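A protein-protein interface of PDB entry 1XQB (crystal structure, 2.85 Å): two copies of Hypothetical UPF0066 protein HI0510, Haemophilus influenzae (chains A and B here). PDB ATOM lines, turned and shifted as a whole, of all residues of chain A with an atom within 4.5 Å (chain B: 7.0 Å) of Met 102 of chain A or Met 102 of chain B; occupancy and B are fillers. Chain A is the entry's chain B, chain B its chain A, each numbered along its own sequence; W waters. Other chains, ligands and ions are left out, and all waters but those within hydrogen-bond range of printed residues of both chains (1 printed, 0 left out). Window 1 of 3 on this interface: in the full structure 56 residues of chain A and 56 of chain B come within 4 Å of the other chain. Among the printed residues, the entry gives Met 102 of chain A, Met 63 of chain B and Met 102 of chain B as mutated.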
ATOM      1  N   TRP A  58     -15.693  27.926 -34.310  1.00  0.00           N
ATOM      2  CA  TRP A  58     -16.777  27.381 -33.491  1.00  0.00           C
ATOM      3  C   TRP A  58     -18.077  27.945 -34.041  1.00  0.00           C
ATOM      4  O   TRP A  58     -18.180  29.145 -34.310  1.00  0.00           O
ATOM      5  CB  TRP A  58     -16.677  27.800 -32.017  1.00  0.00           C
ATOM      6  CG  TRP A  58     -15.860  26.897 -31.112  1.00  0.00           C
ATOM      7  CD1 TRP A  58     -14.761  27.262 -30.405  1.00  0.00           C
ATOM      8  CD2 TRP A  58     -16.123  25.521 -30.760  1.00  0.00           C
ATOM      9  NE1 TRP A  58     -14.325  26.218 -29.632  1.00  0.00           N
ATOM     10  CE2 TRP A  58     -15.140  25.136 -29.828  1.00  0.00           C
ATOM     11  CE3 TRP A  58     -17.092  24.583 -31.138  1.00  0.00           C
ATOM     12  CZ2 TRP A  58     -15.091  23.850 -29.261  1.00  0.00           C
ATOM     13  CZ3 TRP A  58     -17.043  23.287 -30.567  1.00  0.00           C
ATOM     14  CH2 TRP A  58     -16.047  22.943 -29.643  1.00  0.00           C
ATOM     15  N   LEU A  59     -19.039  27.063 -34.266  1.00  0.00           N
ATOM     16  CA  LEU A  59     -20.346  27.473 -34.749  1.00  0.00           C
ATOM     17  C   LEU A  59     -21.376  27.098 -33.687  1.00  0.00           C
ATOM     18  O   LEU A  59     -21.432  25.950 -33.242  1.00  0.00           O
ATOM     19  CB  LEU A  59     -20.706  26.762 -36.055  1.00  0.00           C
ATOM     20  CG  LEU A  59     -19.898  26.922 -37.349  1.00  0.00           C
ATOM     21  CD1 LEU A  59     -20.604  26.158 -38.467  1.00  0.00           C
ATOM     22  CD2 LEU A  59     -19.757  28.383 -37.735  1.00  0.00           C
ATOM     23  N   ILE A  60     -22.107  28.092 -33.197  1.00  0.00           N
ATOM     24  CA  ILE A  60     -23.170  27.834 -32.237  1.00  0.00           C
ATOM     25  C   ILE A  60     -24.426  27.885 -33.119  1.00  0.00           C
ATOM     26  O   ILE A  60     -24.786  28.937 -33.631  1.00  0.00           O
ATOM     27  CB  ILE A  60     -23.190  28.900 -31.111  1.00  0.00           C
ATOM     28  CG1 ILE A  60     -21.882  28.822 -30.310  1.00  0.00           C
ATOM     29  CG2 ILE A  60     -24.398  28.670 -30.180  1.00  0.00           C
ATOM     30  CD1 ILE A  60     -21.637  29.997 -29.359  1.00  0.00           C
ATOM     31  N   PHE A  61     -25.031  26.728 -33.364  1.00  0.00           N
ATOM     32  CA  PHE A  61     -26.194  26.632 -34.249  1.00  0.00           C
ATOM     33  C   PHE A  61     -27.502  26.234 -33.558  1.00  0.00           C
ATOM     34  O   PHE A  61     -27.570  26.126 -32.344  1.00  0.00           O
ATOM     35  CB  PHE A  61     -25.886  25.628 -35.362  1.00  0.00           C
ATOM     36  CG  PHE A  61     -25.639  24.244 -34.861  1.00  0.00           C
ATOM     37  CD1 PHE A  61     -26.632  23.272 -34.941  1.00  0.00           C
ATOM     38  CD2 PHE A  61     -24.431  23.915 -34.265  1.00  0.00           C
ATOM     39  CE1 PHE A  61     -26.426  21.983 -34.429  1.00  0.00           C
ATOM     40  CE2 PHE A  61     -24.208  22.621 -33.744  1.00  0.00           C
ATOM     41  CZ  PHE A  61     -25.212  21.657 -33.829  1.00  0.00           C
ATOM     42  N   ARG A  92     -25.525  14.919 -25.532  1.00  0.00           N
ATOM     43  CA  ARG A  92     -25.478  15.916 -26.604  1.00  0.00           C
ATOM     44  C   ARG A  92     -26.796  15.947 -27.363  1.00  0.00           C
ATOM     45  O   ARG A  92     -26.855  16.418 -28.498  1.00  0.00           O
ATOM     46  CB  ARG A  92     -24.347  15.594 -27.584  1.00  0.00           C
ATOM     47  CG  ARG A  92     -22.973  16.096 -27.173  1.00  0.00           C
ATOM     48  CD  ARG A  92     -22.824  17.604 -27.378  1.00  0.00           C
ATOM     49  NE  ARG A  92     -21.438  18.028 -27.168  1.00  0.00           N
ATOM     50  CZ  ARG A  92     -20.772  18.863 -27.962  1.00  0.00           C
ATOM     51  NH1 ARG A  92     -21.358  19.387 -29.037  1.00  0.00           N
ATOM     52  NH2 ARG A  92     -19.508  19.153 -27.691  1.00  0.00           N
ATOM     53  N   LEU A 100     -29.367  24.840 -28.261  1.00  0.00           N
ATOM     54  CA  LEU A 100     -28.124  25.409 -28.764  1.00  0.00           C
ATOM     55  C   LEU A 100     -27.006  24.388 -28.895  1.00  0.00           C
ATOM     56  O   LEU A 100     -26.528  23.832 -27.911  1.00  0.00           O
ATOM     57  CB  LEU A 100     -27.663  26.572 -27.891  1.00  0.00           C
ATOM     58  CG  LEU A 100     -28.564  27.807 -27.892  1.00  0.00           C
ATOM     59  CD1 LEU A 100     -28.040  28.781 -26.870  1.00  0.00           C
ATOM     60  CD2 LEU A 100     -28.638  28.446 -29.263  1.00  0.00           C
ATOM     61  N   GLY A 101     -26.589  24.151 -30.127  1.00  0.00           N
ATOM     62  CA  GLY A 101     -25.524  23.210 -30.362  1.00  0.00           C
ATOM     63  C   GLY A 101     -24.230  23.889 -30.744  1.00  0.00           C
ATOM     64  O   GLY A 101     -24.211  25.027 -31.227  1.00  0.00           O
ATOM     65  N   MET A 102     -23.140  23.168 -30.501  1.00  0.00           N
ATOM     66  CA  MET A 102     -21.798  23.615 -30.819  1.00  0.00           C
ATOM     67  C   MET A 102     -21.191  22.680 -31.856  1.00  0.00           C
ATOM     68  O   MET A 102     -21.580  21.508 -31.957  1.00  0.00           O
ATOM     69  CB  MET A 102     -20.923  23.569 -29.587  1.00  0.00           C
ATOM     70  CG  MET A 102     -21.260  24.569 -28.532  1.00  0.00           C
ATOM     71  SD  MET A 102     -20.053  24.239 -27.091  1.00  0.00           S
ATOM     72  CE  MET A 102     -20.639  22.439 -26.666  1.00  0.00           C
ATOM     73  N   SER A 103     -20.186  23.184 -32.566  1.00  0.00           N
ATOM     74  CA  SER A 103     -19.511  22.413 -33.592  1.00  0.00           C
ATOM     75  C   SER A 103     -18.243  23.123 -34.070  1.00  0.00           C
ATOM     76  O   SER A 103     -18.292  24.266 -34.535  1.00  0.00           O
ATOM     77  CB  SER A 103     -20.462  22.180 -34.765  1.00  0.00           C
ATOM     78  OG  SER A 103     -19.849  21.415 -35.784  1.00  0.00           O
ATOM     79  N   LYS A 136     -17.300  31.919 -33.731  1.00  0.00           N
ATOM     80  CA  LYS A 136     -16.144  32.260 -32.913  1.00  0.00           C
ATOM     81  C   LYS A 136     -14.906  31.537 -33.421  1.00  0.00           C
ATOM     82  O   LYS A 136     -15.018  30.538 -34.124  1.00  0.00           O
ATOM     83  CB  LYS A 136     -16.386  31.824 -31.472  1.00  0.00           C
ATOM     84  CG  LYS A 136     -17.519  32.501 -30.766  1.00  0.00           C
ATOM     85  CD  LYS A 136     -17.463  32.181 -29.278  1.00  0.00           C
ATOM     86  CE  LYS A 136     -18.621  32.799 -28.513  1.00  0.00           C
ATOM     87  NZ  LYS A 136     -18.708  34.288 -28.583  1.00  0.00           N
ATOM     88  N   TRP B  58     -19.183  21.947 -20.663  1.00  0.00           N
ATOM     89  CA  TRP B  58     -19.272  23.155 -21.481  1.00  0.00           C
ATOM     90  C   TRP B  58     -20.452  23.958 -20.954  1.00  0.00           C
ATOM     91  O   TRP B  58     -21.530  23.416 -20.695  1.00  0.00           O
ATOM     92  CB  TRP B  58     -19.532  22.869 -22.968  1.00  0.00           C
ATOM     93  CG  TRP B  58     -18.317  22.630 -23.836  1.00  0.00           C
ATOM     94  CD1 TRP B  58     -18.038  21.495 -24.524  1.00  0.00           C
ATOM     95  CD2 TRP B  58     -17.276  23.563 -24.173  1.00  0.00           C
ATOM     96  NE1 TRP B  58     -16.903  21.649 -25.271  1.00  0.00           N
ATOM     97  CE2 TRP B  58     -16.410  22.911 -25.079  1.00  0.00           C
ATOM     98  CE3 TRP B  58     -16.991  24.889 -23.807  1.00  0.00           C
ATOM     99  CZ2 TRP B  58     -15.275  23.540 -25.631  1.00  0.00           C
ATOM    100  CZ3 TRP B  58     -15.851  25.521 -24.364  1.00  0.00           C
ATOM    101  CH2 TRP B  58     -15.019  24.844 -25.259  1.00  0.00           C
ATOM    102  N   LEU B  59     -20.216  25.245 -20.746  1.00  0.00           N
ATOM    103  CA  LEU B  59     -21.252  26.151 -20.290  1.00  0.00           C
ATOM    104  C   LEU B  59     -21.459  27.205 -21.375  1.00  0.00           C
ATOM    105  O   LEU B  59     -20.497  27.839 -21.815  1.00  0.00           O
ATOM    106  CB  LEU B  59     -20.841  26.856 -18.994  1.00  0.00           C
ATOM    107  CG  LEU B  59     -20.603  26.094 -17.681  1.00  0.00           C
ATOM    108  CD1 LEU B  59     -20.349  27.112 -16.562  1.00  0.00           C
ATOM    109  CD2 LEU B  59     -21.793  25.193 -17.334  1.00  0.00           C
ATOM    110  N   ILE B  60     -22.688  27.296 -21.882  1.00  0.00           N
ATOM    111  CA  ILE B  60     -23.024  28.320 -22.862  1.00  0.00           C
ATOM    112  C   ILE B  60     -23.737  29.374 -22.000  1.00  0.00           C
ATOM    113  O   ILE B  60     -24.812  29.132 -21.488  1.00  0.00           O
ATOM    114  CB  ILE B  60     -23.929  27.766 -23.986  1.00  0.00           C
ATOM    115  CG1 ILE B  60     -23.155  26.717 -24.792  1.00  0.00           C
ATOM    116  CG2 ILE B  60     -24.363  28.905 -24.923  1.00  0.00           C
ATOM    117  CD1 ILE B  60     -24.014  25.895 -25.753  1.00  0.00           C
ATOM    118  N   PHE B  61     -23.079  30.502 -21.764  1.00  0.00           N
ATOM    119  CA  PHE B  61     -23.624  31.548 -20.899  1.00  0.00           C
ATOM    120  C   PHE B  61     -23.959  32.858 -21.610  1.00  0.00           C
ATOM    121  O   PHE B  61     -23.879  32.955 -22.830  1.00  0.00           O
ATOM    122  CB  PHE B  61     -22.628  31.832 -19.770  1.00  0.00           C
ATOM    123  CG  PHE B  61     -21.300  32.332 -20.248  1.00  0.00           C
ATOM    124  CD1 PHE B  61     -20.993  33.685 -20.196  1.00  0.00           C
ATOM    125  CD2 PHE B  61     -20.373  31.464 -20.791  1.00  0.00           C
ATOM    126  CE1 PHE B  61     -19.775  34.171 -20.685  1.00  0.00           C
ATOM    127  CE2 PHE B  61     -19.143  31.944 -21.287  1.00  0.00           C
ATOM    128  CZ  PHE B  61     -18.850  33.295 -21.232  1.00  0.00           C
ATOM    129  N   MET B  63     -23.099  36.886 -22.158  1.00  0.00           N
ATOM    130  CA  MET B  63     -22.009  37.839 -22.007  1.00  0.00           C
ATOM    131  C   MET B  63     -22.491  39.227 -21.582  1.00  0.00           C
ATOM    132  O   MET B  63     -23.654  39.581 -21.778  1.00  0.00           O
ATOM    133  CB  MET B  63     -21.204  37.924 -23.307  1.00  0.00           C
ATOM    134  CG  MET B  63     -20.636  36.586 -23.782  1.00  0.00           C
ATOM    135  SD  MET B  63     -19.380  36.763 -25.258  1.00  0.00           S
ATOM    136  CE  MET B  63     -20.513  36.288 -26.715  1.00  0.00           C
ATOM    137  N   ARG B  92     -13.129  37.043 -29.491  1.00  0.00           N
ATOM    138  CA  ARG B  92     -13.978  36.487 -28.433  1.00  0.00           C
ATOM    139  C   ARG B  92     -14.717  37.596 -27.694  1.00  0.00           C
ATOM    140  O   ARG B  92     -15.182  37.401 -26.569  1.00  0.00           O
ATOM    141  CB  ARG B  92     -13.133  35.699 -27.429  1.00  0.00           C
ATOM    142  CG  ARG B  92     -12.827  34.264 -27.825  1.00  0.00           C
ATOM    143  CD  ARG B  92     -14.018  33.345 -27.605  1.00  0.00           C
ATOM    144  NE  ARG B  92     -13.646  31.942 -27.796  1.00  0.00           N
ATOM    145  CZ  ARG B  92     -14.008  30.945 -26.993  1.00  0.00           C
ATOM    146  NH1 ARG B  92     -14.766  31.174 -25.923  1.00  0.00           N
ATOM    147  NH2 ARG B  92     -13.597  29.713 -27.255  1.00  0.00           N
ATOM    148  N   LEU B 100     -23.649  35.126 -26.932  1.00  0.00           N
ATOM    149  CA  LEU B 100     -23.485  33.774 -26.408  1.00  0.00           C
ATOM    150  C   LEU B 100     -22.031  33.361 -26.243  1.00  0.00           C
ATOM    151  O   LEU B 100     -21.297  33.228 -27.213  1.00  0.00           O
ATOM    152  CB  LEU B 100     -24.209  32.753 -27.278  1.00  0.00           C
ATOM    153  CG  LEU B 100     -25.730  32.858 -27.323  1.00  0.00           C
ATOM    154  CD1 LEU B 100     -26.242  31.840 -28.302  1.00  0.00           C
ATOM    155  CD2 LEU B 100     -26.348  32.652 -25.962  1.00  0.00           C
ATOM    156  N   GLY B 101     -21.631  33.143 -24.999  1.00  0.00           N
ATOM    157  CA  GLY B 101     -20.278  32.737 -24.724  1.00  0.00           C
ATOM    158  C   GLY B 101     -20.179  31.287 -24.325  1.00  0.00           C
ATOM    159  O   GLY B 101     -21.137  30.687 -23.844  1.00  0.00           O
ATOM    160  N   MET B 102     -18.992  30.735 -24.549  1.00  0.00           N
ATOM    161  CA  MET B 102     -18.661  29.356 -24.219  1.00  0.00           C
ATOM    162  C   MET B 102     -17.570  29.343 -23.167  1.00  0.00           C
ATOM    163  O   MET B 102     -16.778  30.287 -23.065  1.00  0.00           O
ATOM    164  CB  MET B 102     -18.125  28.632 -25.434  1.00  0.00           C
ATOM    165  CG  MET B 102     -19.118  28.375 -26.508  1.00  0.00           C
ATOM    166  SD  MET B 102     -18.152  27.554 -27.939  1.00  0.00           S
ATOM    167  CE  MET B 102     -16.972  29.023 -28.349  1.00  0.00           C
ATOM    168  N   SER B 103     -17.492  28.238 -22.434  1.00  0.00           N
ATOM    169  CA  SER B 103     -16.498  28.080 -21.387  1.00  0.00           C
ATOM    170  C   SER B 103     -16.440  26.634 -20.888  1.00  0.00           C
ATOM    171  O   SER B 103     -17.443  26.080 -20.440  1.00  0.00           O
ATOM    172  CB  SER B 103     -16.811  29.041 -20.236  1.00  0.00           C
ATOM    173  OG  SER B 103     -15.856  28.934 -19.197  1.00  0.00           O
ATOM    174  N   LYS B 104     -15.272  26.012 -21.018  1.00  0.00           N
ATOM    175  CA  LYS B 104     -15.091  24.638 -20.565  1.00  0.00           C
ATOM    176  C   LYS B 104     -14.495  24.623 -19.164  1.00  0.00           C
ATOM    177  O   LYS B 104     -13.355  25.029 -18.949  1.00  0.00           O
ATOM    178  CB  LYS B 104     -14.203  23.843 -21.533  1.00  0.00           C
ATOM    179  CG  LYS B 104     -12.756  24.339 -21.654  1.00  0.00           C
ATOM    180  CD  LYS B 104     -11.754  23.190 -21.609  1.00  0.00           C
ATOM    181  CE  LYS B 104     -10.405  23.706 -21.156  1.00  0.00           C
ATOM    182  NZ  LYS B 104      -9.450  22.600 -20.881  1.00  0.00           N
ATOM    183  N   ASP B 125     -13.946  31.029 -15.183  1.00  0.00           N
ATOM    184  CA  ASP B 125     -13.596  32.364 -15.662  1.00  0.00           C
ATOM    185  C   ASP B 125     -14.805  33.290 -15.891  1.00  0.00           C
ATOM    186  O   ASP B 125     -14.653  34.406 -16.419  1.00  0.00           O
ATOM    187  CB  ASP B 125     -12.764  32.269 -16.948  1.00  0.00           C
ATOM    188  CG  ASP B 125     -13.531  31.653 -18.111  1.00  0.00           C
ATOM    189  OD1 ASP B 125     -14.688  31.208 -17.931  1.00  0.00           O
ATOM    190  OD2 ASP B 125     -12.966  31.608 -19.221  1.00  0.00           O
ATOM    191  N   LEU B 126     -15.996  32.823 -15.512  1.00  0.00           N
ATOM    192  CA  LEU B 126     -17.217  33.614 -15.671  1.00  0.00           C
ATOM    193  C   LEU B 126     -17.408  34.526 -14.461  1.00  0.00           C
ATOM    194  O   LEU B 126     -17.095  34.134 -13.346  1.00  0.00           O
ATOM    195  CB  LEU B 126     -18.425  32.685 -15.819  1.00  0.00           C
ATOM    196  CG  LEU B 126     -18.260  31.532 -16.811  1.00  0.00           C
ATOM    197  CD1 LEU B 126     -19.565  30.765 -16.949  1.00  0.00           C
ATOM    198  CD2 LEU B 126     -17.809  32.076 -18.149  1.00  0.00           C
ATOM    199  N   ASP B 134     -26.864  26.739 -21.307  1.00  0.00           N
ATOM    200  CA  ASP B 134     -26.824  25.310 -21.537  1.00  0.00           C
ATOM    201  C   ASP B 134     -25.628  24.657 -20.875  1.00  0.00           C
ATOM    202  O   ASP B 134     -24.576  25.282 -20.697  1.00  0.00           O
ATOM    203  CB  ASP B 134     -26.820  25.013 -23.036  1.00  0.00           C
ATOM    204  CG  ASP B 134     -27.300  23.620 -23.347  1.00  0.00           C
ATOM    205  OD1 ASP B 134     -26.573  22.857 -24.022  1.00  0.00           O
ATOM    206  OD2 ASP B 134     -28.422  23.288 -22.909  1.00  0.00           O
ATOM    207  N   LYS B 136     -23.427  21.184 -21.296  1.00  0.00           N
ATOM    208  CA  LYS B 136     -23.086  20.015 -22.100  1.00  0.00           C
ATOM    209  C   LYS B 136     -21.835  19.366 -21.561  1.00  0.00           C
ATOM    210  O   LYS B 136     -21.058  20.013 -20.859  1.00  0.00           O
ATOM    211  CB  LYS B 136     -22.800  20.422 -23.540  1.00  0.00           C
ATOM    212  CG  LYS B 136     -23.963  21.011 -24.276  1.00  0.00           C
ATOM    213  CD  LYS B 136     -23.645  21.146 -25.753  1.00  0.00           C
ATOM    214  CE  LYS B 136     -24.812  21.799 -26.503  1.00  0.00           C
ATOM    215  NZ  LYS B 136     -26.083  21.012 -26.473  1.00  0.00           N
ATOM    216  N   PRO B 137     -21.613  18.071 -21.876  1.00  0.00           N
ATOM    217  CA  PRO B 137     -20.407  17.385 -21.398  1.00  0.00           C
ATOM    218  C   PRO B 137     -19.317  17.668 -22.425  1.00  0.00           C
ATOM    219  O   PRO B 137     -19.586  17.642 -23.636  1.00  0.00           O
ATOM    220  CB  PRO B 137     -20.784  15.904 -21.472  1.00  0.00           C
ATOM    221  CG  PRO B 137     -22.216  15.879 -21.897  1.00  0.00           C
ATOM    222  CD  PRO B 137     -22.442  17.138 -22.645  1.00  0.00           C
ATOM    223  N   TYR B 138     -18.105  17.965 -21.965  1.00  0.00           N
ATOM    224  CA  TYR B 138     -17.002  18.215 -22.886  1.00  0.00           C
ATOM    225  C   TYR B 138     -16.456  16.878 -23.338  1.00  0.00           C
ATOM    226  O   TYR B 138     -15.933  16.126 -22.528  1.00  0.00           O
ATOM    227  CB  TYR B 138     -15.902  19.023 -22.198  1.00  0.00           C
ATOM    228  CG  TYR B 138     -14.699  19.307 -23.072  1.00  0.00           C
ATOM    229  CD1 TYR B 138     -14.457  20.591 -23.562  1.00  0.00           C
ATOM    230  CD2 TYR B 138     -13.808  18.291 -23.416  1.00  0.00           C
ATOM    231  CE1 TYR B 138     -13.355  20.850 -24.374  1.00  0.00           C
ATOM    232  CE2 TYR B 138     -12.720  18.531 -24.224  1.00  0.00           C
ATOM    233  CZ  TYR B 138     -12.489  19.806 -24.704  1.00  0.00           C
ATOM    234  OH  TYR B 138     -11.396  20.032 -25.517  1.00  0.00           O
ATOM    235  N   ASP B 143     -14.491  17.900 -29.407  1.00  0.00           N
ATOM    236  CA  ASP B 143     -14.135  19.237 -28.941  1.00  0.00           C
ATOM    237  C   ASP B 143     -12.656  19.574 -28.914  1.00  0.00           C
ATOM    238  O   ASP B 143     -12.293  20.750 -29.002  1.00  0.00           O
ATOM    239  CB  ASP B 143     -14.741  19.513 -27.563  1.00  0.00           C
ATOM    240  CG  ASP B 143     -16.242  19.357 -27.543  1.00  0.00           C
ATOM    241  OD1 ASP B 143     -16.880  19.494 -28.605  1.00  0.00           O
ATOM    242  OD2 ASP B 143     -16.799  19.086 -26.461  1.00  0.00           O
HETATM  243  O   HOH W   1     -17.109  33.500 -25.720  1.00  0.00           O
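Water W1 bridges the guanidinium group (NH1) of Arg 92 of chain B (3.3 Å) and the side-chain amino group (NZ) of Lys 136 of chain A (3.4 Å).
Printed residues of chain B within 4 Å of Trp 58 of chain A: Trp 58, Met 102 and Asp 143.
Printed residues of chain B within 4 Å of Arg 92 of chain A: Lys 136 (3.98 Å) and Asp 143 (2.8 Å).
Printed residues of chain B within 4 Å of Leu 100 of chain A: Ile 60, Leu 100 and Lys 136.
Met 102 of chain A touches just these residues of chain B: Trp 58 (3.5 Å), Met 102 (3.9 Å) and Lys 136 (3.4 Å).
Ser 103 of chain A touches none of the printed residues of chain B.
Of the printed residues of chain A, Trp 58 of chain B touches Trp 58 (3.6 Å) and Met 102 (3.5 Å).
Of chain A, only Trp 58 (3.5 Å), Met 102 (3.9 Å) and Lys 136 (3.3 Å) come within 4 Å of Met 102 of chain B.
Of the printed residues of chain A, Lys 136 of chain B touches Arg 92, Leu 100 and Met 102.
The nearest residue of chain B that does not touch Met 102 of chain A is Ile 60 of chain B (4.1 Å).
NH2 of Arg 92 of chain A is in salt-bridge range of OD1 of Asp 143 of chain B, 2.8 Å away.
O of Leu 100 of chain B sits close to NZ of Lys 136 of chain A, 3.1 Å away.
O of Leu 100 of chain A sits close to NZ of Lys 136 of chain B, at 3.2 Å.
Of the 10 printed residues of chain A, 6 touch a printed residue of chain B.
Hydrophobic or aromatic side chains of chain A that line the printed part of chain B: Trp 58, Ile 60, Leu 100 and Met 102.
Among the printed residues, Asp or Glu carboxylates within 4 Å of a Lys or Arg side-chain nitrogen of the other chain: Arg 92 of chain A with Asp 143 of chain B (2.8 Å).
Trp 58 of chain A touches Trp 58 of chain B.
CD1 of Trp 58 of chain A touches CE of Met 102 of chain B, 3.5 Å away.
Trp 58 of chain A touches Asp 143 of chain B.
Lys 136 of chain B touches Arg 92 of chain A.
Leu 100 of chain B touches Leu 100 of chain A (CD1 to CD1, 3.8 Å).
CE of Met 102 of chain A touches CD1 of Trp 58 of chain B (3.5 Å).
Met 102 of chain A touches Met 102 of chain B.
CE of Met 102 of chain A touches CD of Lys 136 of chain B, 3.4 Å away.
Met 63 of chain B touches Lys 136 of chain A (CE to NZ, 3.3 Å).
Lys 136 of chain A touches Met 102 of chain B.
Trp 58 of chain B touches its own counterpart, Trp 58 of chain A.
Trp 58 of chain A touches Met 102 of chain B, and with the chains exchanged Met 102 of chain A touches Trp 58 of chain B.
Ile 60 of chain A touches Leu 100 of chain B, and with the chains exchanged Leu 100 of chain A touches Ile 60 of chain B.
Met 102 of chain A touches Lys 136 of chain B, and with the chains exchanged Lys 136 of chain A touches Met 102 of chain B.
Positions printed for both chains: 58, 59, 60, 61, 92, 100, 101, 102, 103 and 136.
Of the 15 pairs that touch across the chains among the printed residues, 11 have their exchanged pair printed and touching as well.
The side-chain carboxylate (OD2) of Asp 143 of chain B lies within hydrogen-bond range of the indole nitrogen (NE1) of Trp 58 of chain B, 2.8 Å away.
O of Lys 136 of chain B lies within hydrogen-bond range of N of Trp 58 of chain B, at 2.7 Å.
The side-chain amino group (NZ) of Lys 136 of chain B lies within salt-bridge range of the side-chain carboxylate (OD1) of Asp 134 of chain B (3.1 Å).
N of Ile 60 of chain B is in hydrogen-bond range of O of Asp 134 of chain B.
The backbone NH of Trp 58 of chain A sits at hydrogen-bond distance from the backbone carbonyl oxygen of Lys 136 of chain A, 2.7 Å away.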
